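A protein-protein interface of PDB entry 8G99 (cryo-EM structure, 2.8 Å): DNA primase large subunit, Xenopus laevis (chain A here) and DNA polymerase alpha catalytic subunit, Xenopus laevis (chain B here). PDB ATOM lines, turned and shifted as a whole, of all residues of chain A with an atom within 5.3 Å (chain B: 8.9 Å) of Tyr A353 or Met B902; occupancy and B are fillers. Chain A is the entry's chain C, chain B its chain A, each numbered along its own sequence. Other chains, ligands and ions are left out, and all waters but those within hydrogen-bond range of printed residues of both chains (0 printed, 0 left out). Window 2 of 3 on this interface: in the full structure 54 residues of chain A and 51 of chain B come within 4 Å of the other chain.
The side-chain carboxylate (OD2) of Asp B896 lies within hydrogen-bond range of the side-chain hydroxyl (OH) of Tyr A353 (3.2 Å).
The side-chain carboxylate (OD1) of Asp B896 is in hydrogen-bond range of the backbone NH (N) of Leu B899, 2.7 Å away.
OH of Tyr A353 touches CB of Ala B898, 3.7 Å away. Leu B899 touches Tyr A353. SD of Met B902 touches CD2 of Tyr A353, 3.7 Å away. NE2 of His A357 touches OD2 of Asp B896, 3.7 Å away.
Tyr A353 touches four residues of chain B. Printed residues of chain A within 4 Å of Met B902: Tyr A353. No residue of chain B comes within 4 Å of Ala A352. Of the printed residues of chain B, His A357 touches Asp B896. Of the printed residues of chain A, Leu B899 touches Tyr A353. Of the printed residues of chain A, Asp B896 touches Tyr A353 (3.2 Å) and His A357 (3.7 Å). Of the printed residues of chain A, Ala B898 touches Tyr A353. The nearest residue of chain B that does not touch Tyr A353 is Gly B894 (5.0 Å).
Of the 25 printed residues of chain B, 4 touch a printed residue of chain A. Printed residues of chain B that touch a printed residue of chain A: Asp B896, Ala B898, Leu B899 and Met B902. Printed residues of chain A that touch a printed residue of chain B: Tyr A353 and His A357. Among the printed residues, 5 pairs touch across the chains.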
ATOM      1  N   PHE A 347      -2.706  36.287 -25.780  1.00  0.00           N
ATOM      2  CA  PHE A 347      -1.662  35.746 -26.640  1.00  0.00           C
ATOM      3  C   PHE A 347      -0.726  34.844 -25.857  1.00  0.00           C
ATOM      4  O   PHE A 347      -0.182  33.881 -26.410  1.00  0.00           O
ATOM      5  CB  PHE A 347      -0.879  36.878 -27.300  1.00  0.00           C
ATOM      6  CG  PHE A 347       0.029  36.419 -28.403  1.00  0.00           C
ATOM      7  CD1 PHE A 347       1.310  35.978 -28.123  1.00  0.00           C
ATOM      8  CD2 PHE A 347      -0.398  36.423 -29.717  1.00  0.00           C
ATOM      9  CE1 PHE A 347       2.146  35.553 -29.131  1.00  0.00           C
ATOM     10  CE2 PHE A 347       0.434  35.998 -30.730  1.00  0.00           C
ATOM     11  CZ  PHE A 347       1.708  35.563 -30.436  1.00  0.00           C
ATOM     12  N   ASP A 348      -0.526  35.132 -24.571  1.00  0.00           N
ATOM     13  CA  ASP A 348       0.357  34.298 -23.769  1.00  0.00           C
ATOM     14  C   ASP A 348      -0.309  32.991 -23.375  1.00  0.00           C
ATOM     15  O   ASP A 348       0.376  31.978 -23.194  1.00  0.00           O
ATOM     16  CB  ASP A 348       0.801  35.057 -22.519  1.00  0.00           C
ATOM     17  CG  ASP A 348       1.632  36.280 -22.846  1.00  0.00           C
ATOM     18  OD1 ASP A 348       2.117  36.383 -23.992  1.00  0.00           O
ATOM     19  OD2 ASP A 348       1.802  37.141 -21.956  1.00  0.00           O
ATOM     20  N   VAL A 350      -3.254  31.339 -24.894  1.00  0.00           N
ATOM     21  CA  VAL A 350      -3.897  30.510 -25.907  1.00  0.00           C
ATOM     22  C   VAL A 350      -2.976  30.258 -27.096  1.00  0.00           C
ATOM     23  O   VAL A 350      -2.813  29.118 -27.533  1.00  0.00           O
ATOM     24  CB  VAL A 350      -5.231  31.142 -26.367  1.00  0.00           C
ATOM     25  CG1 VAL A 350      -5.820  30.358 -27.530  1.00  0.00           C
ATOM     26  CG2 VAL A 350      -6.214  31.206 -25.208  1.00  0.00           C
ATOM     27  N   TYR A 351      -2.361  31.312 -27.631  1.00  0.00           N
ATOM     28  CA  TYR A 351      -1.671  31.232 -28.912  1.00  0.00           C
ATOM     29  C   TYR A 351      -0.169  31.021 -28.801  1.00  0.00           C
ATOM     30  O   TYR A 351       0.405  30.335 -29.652  1.00  0.00           O
ATOM     31  CB  TYR A 351      -1.925  32.509 -29.721  1.00  0.00           C
ATOM     32  CG  TYR A 351      -3.348  32.669 -30.206  1.00  0.00           C
ATOM     33  CD1 TYR A 351      -4.057  31.592 -30.718  1.00  0.00           C
ATOM     34  CD2 TYR A 351      -3.981  33.899 -30.150  1.00  0.00           C
ATOM     35  CE1 TYR A 351      -5.356  31.739 -31.161  1.00  0.00           C
ATOM     36  CE2 TYR A 351      -5.277  34.056 -30.591  1.00  0.00           C
ATOM     37  CZ  TYR A 351      -5.961  32.973 -31.095  1.00  0.00           C
ATOM     38  OH  TYR A 351      -7.255  33.126 -31.535  1.00  0.00           O
ATOM     39  N   ALA A 352       0.485  31.588 -27.785  1.00  0.00           N
ATOM     40  CA  ALA A 352       1.945  31.558 -27.734  1.00  0.00           C
ATOM     41  C   ALA A 352       2.476  30.136 -27.877  1.00  0.00           C
ATOM     42  O   ALA A 352       3.379  29.873 -28.681  1.00  0.00           O
ATOM     43  CB  ALA A 352       2.434  32.184 -26.428  1.00  0.00           C
ATOM     44  N   TYR A 353       1.907  29.201 -27.119  1.00  0.00           N
ATOM     45  CA  TYR A 353       2.388  27.828 -27.176  1.00  0.00           C
ATOM     46  C   TYR A 353       2.455  27.335 -28.611  1.00  0.00           C
ATOM     47  O   TYR A 353       3.421  26.674 -29.003  1.00  0.00           O
ATOM     48  CB  TYR A 353       1.486  26.916 -26.346  1.00  0.00           C
ATOM     49  CG  TYR A 353       1.934  25.471 -26.330  1.00  0.00           C
ATOM     50  CD1 TYR A 353       1.490  24.576 -27.292  1.00  0.00           C
ATOM     51  CD2 TYR A 353       2.798  25.003 -25.351  1.00  0.00           C
ATOM     52  CE1 TYR A 353       1.896  23.255 -27.282  1.00  0.00           C
ATOM     53  CE2 TYR A 353       3.208  23.683 -25.332  1.00  0.00           C
ATOM     54  CZ  TYR A 353       2.755  22.815 -26.299  1.00  0.00           C
ATOM     55  OH  TYR A 353       3.160  21.501 -26.285  1.00  0.00           O
ATOM     56  N   SER A 354       1.424  27.625 -29.404  1.00  0.00           N
ATOM     57  CA  SER A 354       1.442  27.224 -30.804  1.00  0.00           C
ATOM     58  C   SER A 354       2.764  27.616 -31.445  1.00  0.00           C
ATOM     59  O   SER A 354       3.523  26.759 -31.910  1.00  0.00           O
ATOM     60  CB  SER A 354       0.265  27.857 -31.546  1.00  0.00           C
ATOM     61  OG  SER A 354      -0.969  27.478 -30.962  1.00  0.00           O
ATOM     62  N   ILE A 355       3.074  28.913 -31.435  1.00  0.00           N
ATOM     63  CA  ILE A 355       4.305  29.379 -32.060  1.00  0.00           C
ATOM     64  C   ILE A 355       5.500  28.651 -31.466  1.00  0.00           C
ATOM     65  O   ILE A 355       6.406  28.208 -32.190  1.00  0.00           O
ATOM     66  CB  ILE A 355       4.433  30.906 -31.905  1.00  0.00           C
ATOM     67  CG1 ILE A 355       3.255  31.606 -32.584  1.00  0.00           C
ATOM     68  CG2 ILE A 355       5.740  31.393 -32.497  1.00  0.00           C
ATOM     69  CD1 ILE A 355       2.323  32.298 -31.626  1.00  0.00           C
ATOM     70  N   ARG A 356       5.515  28.488 -30.143  1.00  0.00           N
ATOM     71  CA  ARG A 356       6.654  27.826 -29.525  1.00  0.00           C
ATOM     72  C   ARG A 356       6.855  26.450 -30.139  1.00  0.00           C
ATOM     73  O   ARG A 356       7.968  26.083 -30.534  1.00  0.00           O
ATOM     74  CB  ARG A 356       6.448  27.733 -28.014  1.00  0.00           C
ATOM     75  CG  ARG A 356       7.192  28.806 -27.239  1.00  0.00           C
ATOM     76  CD  ARG A 356       6.867  28.764 -25.759  1.00  0.00           C
ATOM     77  NE  ARG A 356       6.183  29.973 -25.317  1.00  0.00           N
ATOM     78  CZ  ARG A 356       6.739  31.174 -25.272  1.00  0.00           C
ATOM     79  NH1 ARG A 356       7.998  31.369 -25.629  1.00  0.00           N
ATOM     80  NH2 ARG A 356       6.014  32.209 -24.859  1.00  0.00           N
ATOM     81  N   HIS A 357       5.766  25.697 -30.278  1.00  0.00           N
ATOM     82  CA  HIS A 357       5.853  24.369 -30.870  1.00  0.00           C
ATOM     83  C   HIS A 357       6.310  24.461 -32.316  1.00  0.00           C
ATOM     84  O   HIS A 357       7.102  23.635 -32.784  1.00  0.00           O
ATOM     85  CB  HIS A 357       4.501  23.665 -30.771  1.00  0.00           C
ATOM     86  CG  HIS A 357       4.597  22.175 -30.705  1.00  0.00           C
ATOM     87  ND1 HIS A 357       3.876  21.345 -31.533  1.00  0.00           N
ATOM     88  CD2 HIS A 357       5.330  21.364 -29.906  1.00  0.00           C
ATOM     89  CE1 HIS A 357       4.160  20.087 -31.250  1.00  0.00           C
ATOM     90  NE2 HIS A 357       5.040  20.071 -30.266  1.00  0.00           N
ATOM     91  N   ASN A 358       5.825  25.473 -33.036  1.00  0.00           N
ATOM     92  CA  ASN A 358       6.271  25.679 -34.405  1.00  0.00           C
ATOM     93  C   ASN A 358       7.780  25.805 -34.467  1.00  0.00           C
ATOM     94  O   ASN A 358       8.399  25.393 -35.453  1.00  0.00           O
ATOM     95  CB  ASN A 358       5.615  26.922 -35.003  1.00  0.00           C
ATOM     96  CG  ASN A 358       4.166  26.698 -35.366  1.00  0.00           C
ATOM     97  OD1 ASN A 358       3.655  25.584 -35.271  1.00  0.00           O
ATOM     98  ND2 ASN A 358       3.493  27.761 -35.788  1.00  0.00           N
ATOM     99  N   GLN B 778      -9.037  25.047 -22.595  1.00  0.00           N
ATOM    100  CA  GLN B 778      -7.905  25.574 -21.840  1.00  0.00           C
ATOM    101  C   GLN B 778      -8.372  26.235 -20.552  1.00  0.00           C
ATOM    102  O   GLN B 778      -7.771  26.038 -19.487  1.00  0.00           O
ATOM    103  CB  GLN B 778      -7.123  26.566 -22.699  1.00  0.00           C
ATOM    104  CG  GLN B 778      -5.923  27.181 -22.002  1.00  0.00           C
ATOM    105  CD  GLN B 778      -6.267  28.452 -21.251  1.00  0.00           C
ATOM    106  OE1 GLN B 778      -7.234  29.139 -21.577  1.00  0.00           O
ATOM    107  NE2 GLN B 778      -5.472  28.771 -20.237  1.00  0.00           N
ATOM    108  N   LEU B 781      -9.365  23.477 -18.033  1.00  0.00           N
ATOM    109  CA  LEU B 781      -8.238  22.702 -17.530  1.00  0.00           C
ATOM    110  C   LEU B 781      -7.389  23.524 -16.569  1.00  0.00           C
ATOM    111  O   LEU B 781      -6.965  23.020 -15.521  1.00  0.00           O
ATOM    112  CB  LEU B 781      -7.399  22.176 -18.691  1.00  0.00           C
ATOM    113  CG  LEU B 781      -8.072  21.125 -19.581  1.00  0.00           C
ATOM    114  CD1 LEU B 781      -7.057  20.510 -20.517  1.00  0.00           C
ATOM    115  CD2 LEU B 781      -8.760  20.042 -18.768  1.00  0.00           C
ATOM    116  N   THR B 782      -7.135  24.794 -16.896  1.00  0.00           N
ATOM    117  CA  THR B 782      -6.405  25.648 -15.966  1.00  0.00           C
ATOM    118  C   THR B 782      -7.179  25.824 -14.666  1.00  0.00           C
ATOM    119  O   THR B 782      -6.595  25.805 -13.576  1.00  0.00           O
ATOM    120  CB  THR B 782      -6.118  27.005 -16.610  1.00  0.00           C
ATOM    121  OG1 THR B 782      -5.303  26.819 -17.772  1.00  0.00           O
ATOM    122  CG2 THR B 782      -5.397  27.920 -15.634  1.00  0.00           C
ATOM    123  N   GLY B 785      -6.800  22.609 -12.625  1.00  0.00           N
ATOM    124  CA  GLY B 785      -5.469  22.510 -12.050  1.00  0.00           C
ATOM    125  C   GLY B 785      -5.285  23.438 -10.866  1.00  0.00           C
ATOM    126  O   GLY B 785      -4.752  23.044  -9.823  1.00  0.00           O
ATOM    127  N   GLU B 786      -5.736  24.687 -11.007  1.00  0.00           N
ATOM    128  CA  GLU B 786      -5.619  25.637  -9.907  1.00  0.00           C
ATOM    129  C   GLU B 786      -6.457  25.204  -8.714  1.00  0.00           C
ATOM    130  O   GLU B 786      -6.028  25.345  -7.564  1.00  0.00           O
ATOM    131  CB  GLU B 786      -6.030  27.032 -10.375  1.00  0.00           C
ATOM    132  CG  GLU B 786      -4.942  27.766 -11.139  1.00  0.00           C
ATOM    133  CD  GLU B 786      -5.463  28.988 -11.870  1.00  0.00           C
ATOM    134  OE1 GLU B 786      -6.643  29.344 -11.671  1.00  0.00           O
ATOM    135  OE2 GLU B 786      -4.691  29.594 -12.643  1.00  0.00           O
ATOM    136  N   LEU B 877      -3.626  14.742 -11.186  1.00  0.00           N
ATOM    137  CA  LEU B 877      -3.625  15.527 -12.412  1.00  0.00           C
ATOM    138  C   LEU B 877      -2.917  14.838 -13.567  1.00  0.00           C
ATOM    139  O   LEU B 877      -3.276  15.072 -14.724  1.00  0.00           O
ATOM    140  CB  LEU B 877      -2.968  16.890 -12.170  1.00  0.00           C
ATOM    141  CG  LEU B 877      -3.693  17.855 -11.231  1.00  0.00           C
ATOM    142  CD1 LEU B 877      -2.986  19.194 -11.220  1.00  0.00           C
ATOM    143  CD2 LEU B 877      -5.146  18.028 -11.631  1.00  0.00           C
ATOM    144  N   HIS B 882      -5.459  13.895 -16.808  1.00  0.00           N
ATOM    145  CA  HIS B 882      -4.768  14.038 -18.086  1.00  0.00           C
ATOM    146  C   HIS B 882      -5.135  12.944 -19.074  1.00  0.00           C
ATOM    147  O   HIS B 882      -5.373  13.265 -20.250  1.00  0.00           O
ATOM    148  CB  HIS B 882      -3.257  14.084 -17.855  1.00  0.00           C
ATOM    149  CG  HIS B 882      -2.465  14.244 -19.112  1.00  0.00           C
ATOM    150  ND1 HIS B 882      -2.233  13.202 -19.981  1.00  0.00           N
ATOM    151  CD2 HIS B 882      -1.854  15.324 -19.650  1.00  0.00           C
ATOM    152  CE1 HIS B 882      -1.512  13.631 -20.999  1.00  0.00           C
ATOM    153  NE2 HIS B 882      -1.267  14.916 -20.822  1.00  0.00           N
ATOM    154  N   GLY B 894      -3.202  20.776 -33.146  1.00  0.00           N
ATOM    155  CA  GLY B 894      -2.716  21.869 -32.337  1.00  0.00           C
ATOM    156  C   GLY B 894      -2.744  21.606 -30.848  1.00  0.00           C
ATOM    157  O   GLY B 894      -2.192  22.407 -30.086  1.00  0.00           O
ATOM    158  N   ILE B 895      -3.368  20.515 -30.414  1.00  0.00           N
ATOM    159  CA  ILE B 895      -3.399  20.115 -29.014  1.00  0.00           C
ATOM    160  C   ILE B 895      -2.702  18.770 -28.895  1.00  0.00           C
ATOM    161  O   ILE B 895      -3.016  17.835 -29.639  1.00  0.00           O
ATOM    162  CB  ILE B 895      -4.838  20.036 -28.473  1.00  0.00           C
ATOM    163  CG1 ILE B 895      -5.551  21.371 -28.682  1.00  0.00           C
ATOM    164  CG2 ILE B 895      -4.835  19.661 -26.995  1.00  0.00           C
ATOM    165  CD1 ILE B 895      -6.901  21.459 -28.008  1.00  0.00           C
ATOM    166  N   ASP B 896      -1.756  18.677 -27.966  1.00  0.00           N
ATOM    167  CA  ASP B 896      -1.042  17.444 -27.683  1.00  0.00           C
ATOM    168  C   ASP B 896      -1.092  17.177 -26.183  1.00  0.00           C
ATOM    169  O   ASP B 896      -1.601  17.984 -25.401  1.00  0.00           O
ATOM    170  CB  ASP B 896       0.407  17.515 -28.181  1.00  0.00           C
ATOM    171  CG  ASP B 896       1.150  18.720 -27.648  1.00  0.00           C
ATOM    172  OD1 ASP B 896       0.562  19.480 -26.852  1.00  0.00           O
ATOM    173  OD2 ASP B 896       2.326  18.910 -28.026  1.00  0.00           O
ATOM    174  N   SER B 897      -0.557  16.022 -25.784  1.00  0.00           N
ATOM    175  CA  SER B 897      -0.525  15.673 -24.369  1.00  0.00           C
ATOM    176  C   SER B 897       0.287  16.688 -23.576  1.00  0.00           C
ATOM    177  O   SER B 897      -0.073  17.036 -22.445  1.00  0.00           O
ATOM    178  CB  SER B 897       0.051  14.270 -24.195  1.00  0.00           C
ATOM    179  OG  SER B 897      -0.717  13.314 -24.903  1.00  0.00           O
ATOM    180  N   ALA B 898       1.388  17.171 -24.152  1.00  0.00           N
ATOM    181  CA  ALA B 898       2.211  18.158 -23.466  1.00  0.00           C
ATOM    182  C   ALA B 898       1.435  19.442 -23.207  1.00  0.00           C
ATOM    183  O   ALA B 898       1.546  20.035 -22.129  1.00  0.00           O
ATOM    184  CB  ALA B 898       3.467  18.448 -24.285  1.00  0.00           C
ATOM    185  N   LEU B 899       0.648  19.893 -24.185  1.00  0.00           N
ATOM    186  CA  LEU B 899      -0.124  21.116 -23.999  1.00  0.00           C
ATOM    187  C   LEU B 899      -1.169  20.944 -22.905  1.00  0.00           C
ATOM    188  O   LEU B 899      -1.384  21.851 -22.092  1.00  0.00           O
ATOM    189  CB  LEU B 899      -0.785  21.521 -25.316  1.00  0.00           C
ATOM    190  CG  LEU B 899      -1.623  22.799 -25.300  1.00  0.00           C
ATOM    191  CD1 LEU B 899      -0.871  23.937 -24.630  1.00  0.00           C
ATOM    192  CD2 LEU B 899      -2.028  23.178 -26.711  1.00  0.00           C
ATOM    193  N   ILE B 900      -1.833  19.790 -22.872  1.00  0.00           N
ATOM    194  CA  ILE B 900      -2.828  19.540 -21.836  1.00  0.00           C
ATOM    195  C   ILE B 900      -2.166  19.497 -20.466  1.00  0.00           C
ATOM    196  O   ILE B 900      -2.699  20.027 -19.484  1.00  0.00           O
ATOM    197  CB  ILE B 900      -3.597  18.242 -22.140  1.00  0.00           C
ATOM    198  CG1 ILE B 900      -4.477  18.431 -23.373  1.00  0.00           C
ATOM    199  CG2 ILE B 900      -4.438  17.831 -20.945  1.00  0.00           C
ATOM    200  CD1 ILE B 900      -4.842  17.144 -24.058  1.00  0.00           C
ATOM    201  N   ALA B 901      -0.995  18.863 -20.378  1.00  0.00           N
ATOM    202  CA  ALA B 901      -0.265  18.841 -19.116  1.00  0.00           C
ATOM    203  C   ALA B 901       0.113  20.249 -18.679  1.00  0.00           C
ATOM    204  O   ALA B 901      -0.004  20.595 -17.499  1.00  0.00           O
ATOM    205  CB  ALA B 901       0.981  17.967 -19.248  1.00  0.00           C
ATOM    206  N   MET B 902       0.569  21.075 -19.621  1.00  0.00           N
ATOM    207  CA  MET B 902       0.911  22.454 -19.296  1.00  0.00           C
ATOM    208  C   MET B 902      -0.304  23.208 -18.775  1.00  0.00           C
ATOM    209  O   MET B 902      -0.215  23.938 -17.782  1.00  0.00           O
ATOM    210  CB  MET B 902       1.483  23.149 -20.530  1.00  0.00           C
ATOM    211  CG  MET B 902       2.136  24.488 -20.254  1.00  0.00           C
ATOM    212  SD  MET B 902       2.156  25.545 -21.711  1.00  0.00           S
ATOM    213  CE  MET B 902       1.296  26.991 -21.098  1.00  0.00           C
ATOM    214  N   TRP B 903      -1.452  23.042 -19.432  1.00  0.00           N
ATOM    215  CA  TRP B 903      -2.661  23.722 -18.984  1.00  0.00           C
ATOM    216  C   TRP B 903      -3.071  23.255 -17.593  1.00  0.00           C
ATOM    217  O   TRP B 903      -3.507  24.061 -16.763  1.00  0.00           O
ATOM    218  CB  TRP B 903      -3.794  23.494 -19.982  1.00  0.00           C
ATOM    219  CG  TRP B 903      -3.616  24.221 -21.281  1.00  0.00           C
ATOM    220  CD1 TRP B 903      -2.775  25.263 -21.530  1.00  0.00           C
ATOM    221  CD2 TRP B 903      -4.297  23.957 -22.512  1.00  0.00           C
ATOM    222  NE1 TRP B 903      -2.889  25.665 -22.836  1.00  0.00           N
ATOM    223  CE2 TRP B 903      -3.819  24.877 -23.461  1.00  0.00           C
ATOM    224  CE3 TRP B 903      -5.266  23.029 -22.903  1.00  0.00           C
ATOM    225  CZ2 TRP B 903      -4.275  24.898 -24.773  1.00  0.00           C
ATOM    226  CZ3 TRP B 903      -5.717  23.053 -24.205  1.00  0.00           C
ATOM    227  CH2 TRP B 903      -5.223  23.980 -25.125  1.00  0.00           C
ATOM    228  N   LEU B 904      -2.946  21.955 -17.318  1.00  0.00           N
ATOM    229  CA  LEU B 904      -3.274  21.445 -15.991  1.00  0.00           C
ATOM    230  C   LEU B 904      -2.292  21.924 -14.930  1.00  0.00           C
ATOM    231  O   LEU B 904      -2.612  21.866 -13.740  1.00  0.00           O
ATOM    232  CB  LEU B 904      -3.306  19.917 -16.000  1.00  0.00           C
ATOM    233  CG  LEU B 904      -4.508  19.249 -16.669  1.00  0.00           C
ATOM    234  CD1 LEU B 904      -4.383  17.740 -16.588  1.00  0.00           C
ATOM    235  CD2 LEU B 904      -5.810  19.706 -16.045  1.00  0.00           C
ATOM    236  N   GLY B 905      -1.114  22.390 -15.330  1.00  0.00           N
ATOM    237  CA  GLY B 905      -0.109  22.843 -14.395  1.00  0.00           C
ATOM    238  C   GLY B 905       1.021  21.873 -14.143  1.00  0.00           C
ATOM    239  O   GLY B 905       1.787  22.078 -13.195  1.00  0.00           O
ATOM    240  N   LEU B 906       1.150  20.829 -14.951  1.00  0.00           N
ATOM    241  CA  LEU B 906       2.184  19.826 -14.765  1.00  0.00           C
ATOM    242  C   LEU B 906       3.424  20.214 -15.568  1.00  0.00           C
ATOM    243  O   LEU B 906       3.532  21.327 -16.090  1.00  0.00           O
ATOM    244  CB  LEU B 906       1.660  18.450 -15.164  1.00  0.00           C
ATOM    245  CG  LEU B 906       0.420  17.971 -14.412  1.00  0.00           C
ATOM    246  CD1 LEU B 906      -0.262  16.856 -15.180  1.00  0.00           C
ATOM    247  CD2 LEU B 906       0.790  17.513 -13.012  1.00  0.00           C
ATOM    248  N   ASP B 907       4.380  19.291 -15.673  1.00  0.00           N
ATOM    249  CA  ASP B 907       5.598  19.523 -16.432  1.00  0.00           C
ATOM    250  C   ASP B 907       5.470  18.849 -17.788  1.00  0.00           C
ATOM    251  O   ASP B 907       5.414  17.611 -17.846  1.00  0.00           O
ATOM    252  CB  ASP B 907       6.811  18.982 -15.682  1.00  0.00           C
ATOM    253  CG  ASP B 907       8.109  19.611 -16.142  1.00  0.00           C
ATOM    254  OD1 ASP B 907       8.229  19.915 -17.348  1.00  0.00           O
ATOM    255  OD2 ASP B 907       9.012  19.802 -15.299  1.00  0.00           O
ATOM    256  N   PRO B 908       5.420  19.593 -18.895  1.00  0.00           N
ATOM    257  CA  PRO B 908       5.286  18.939 -20.206  1.00  0.00           C
ATOM    258  C   PRO B 908       6.434  18.008 -20.542  1.00  0.00           C
ATOM    259  O   PRO B 908       6.268  17.129 -21.397  1.00  0.00           O
ATOM    260  CB  PRO B 908       5.220  20.120 -21.184  1.00  0.00           C
ATOM    261  CG  PRO B 908       4.797  21.280 -20.364  1.00  0.00           C
ATOM    262  CD  PRO B 908       5.371  21.061 -19.006  1.00  0.00           C
ATOM    263  N   SER B 909       7.595  18.170 -19.904  1.00  0.00           N
ATOM    264  CA  SER B 909       8.732  17.308 -20.209  1.00  0.00           C
ATOM    265  C   SER B 909       8.399  15.838 -19.996  1.00  0.00           C
ATOM    266  O   SER B 909       8.920  14.974 -20.709  1.00  0.00           O
ATOM    267  CB  SER B 909       9.932  17.705 -19.350  1.00  0.00           C
ATOM    268  OG  SER B 909      10.361  19.022 -19.650  1.00  0.00           O
ATOM    269  N   PHE B 911       5.594  14.312 -20.535  1.00  0.00           N
ATOM    270  CA  PHE B 911       4.558  13.816 -21.429  1.00  0.00           C
ATOM    271  C   PHE B 911       4.966  13.817 -22.894  1.00  0.00           C
ATOM    272  O   PHE B 911       4.246  13.240 -23.717  1.00  0.00           O
ATOM    273  CB  PHE B 911       3.280  14.648 -21.265  1.00  0.00           C
ATOM    274  CG  PHE B 911       2.630  14.496 -19.924  1.00  0.00           C
ATOM    275  CD1 PHE B 911       1.703  13.497 -19.699  1.00  0.00           C
ATOM    276  CD2 PHE B 911       2.952  15.350 -18.887  1.00  0.00           C
ATOM    277  CE1 PHE B 911       1.105  13.356 -18.465  1.00  0.00           C
ATOM    278  CE2 PHE B 911       2.357  15.213 -17.652  1.00  0.00           C
ATOM    279  CZ  PHE B 911       1.433  14.215 -17.442  1.00  0.00           C
ATOM    280  N   ARG B 912       6.084  14.442 -23.244  1.00  0.00           N
ATOM    281  CA  ARG B 912       6.539  14.466 -24.627  1.00  0.00           C
ATOM    282  C   ARG B 912       6.922  13.066 -25.089  1.00  0.00           C
ATOM    283  O   ARG B 912       8.104  12.730 -25.172  1.00  0.00           O
ATOM    284  CB  ARG B 912       7.727  15.417 -24.786  1.00  0.00           C
ATOM    285  CG  ARG B 912       7.354  16.889 -24.705  1.00  0.00           C
ATOM    286  CD  ARG B 912       8.588  17.777 -24.719  1.00  0.00           C
ATOM    287  NE  ARG B 912       8.244  19.191 -24.628  1.00  0.00           N
ATOM    288  CZ  ARG B 912       9.128  20.180 -24.605  1.00  0.00           C
ATOM    289  NH1 ARG B 912      10.429  19.945 -24.663  1.00  0.00           N
ATOM    290  NH2 ARG B 912       8.696  21.434 -24.521  1.00  0.00           N
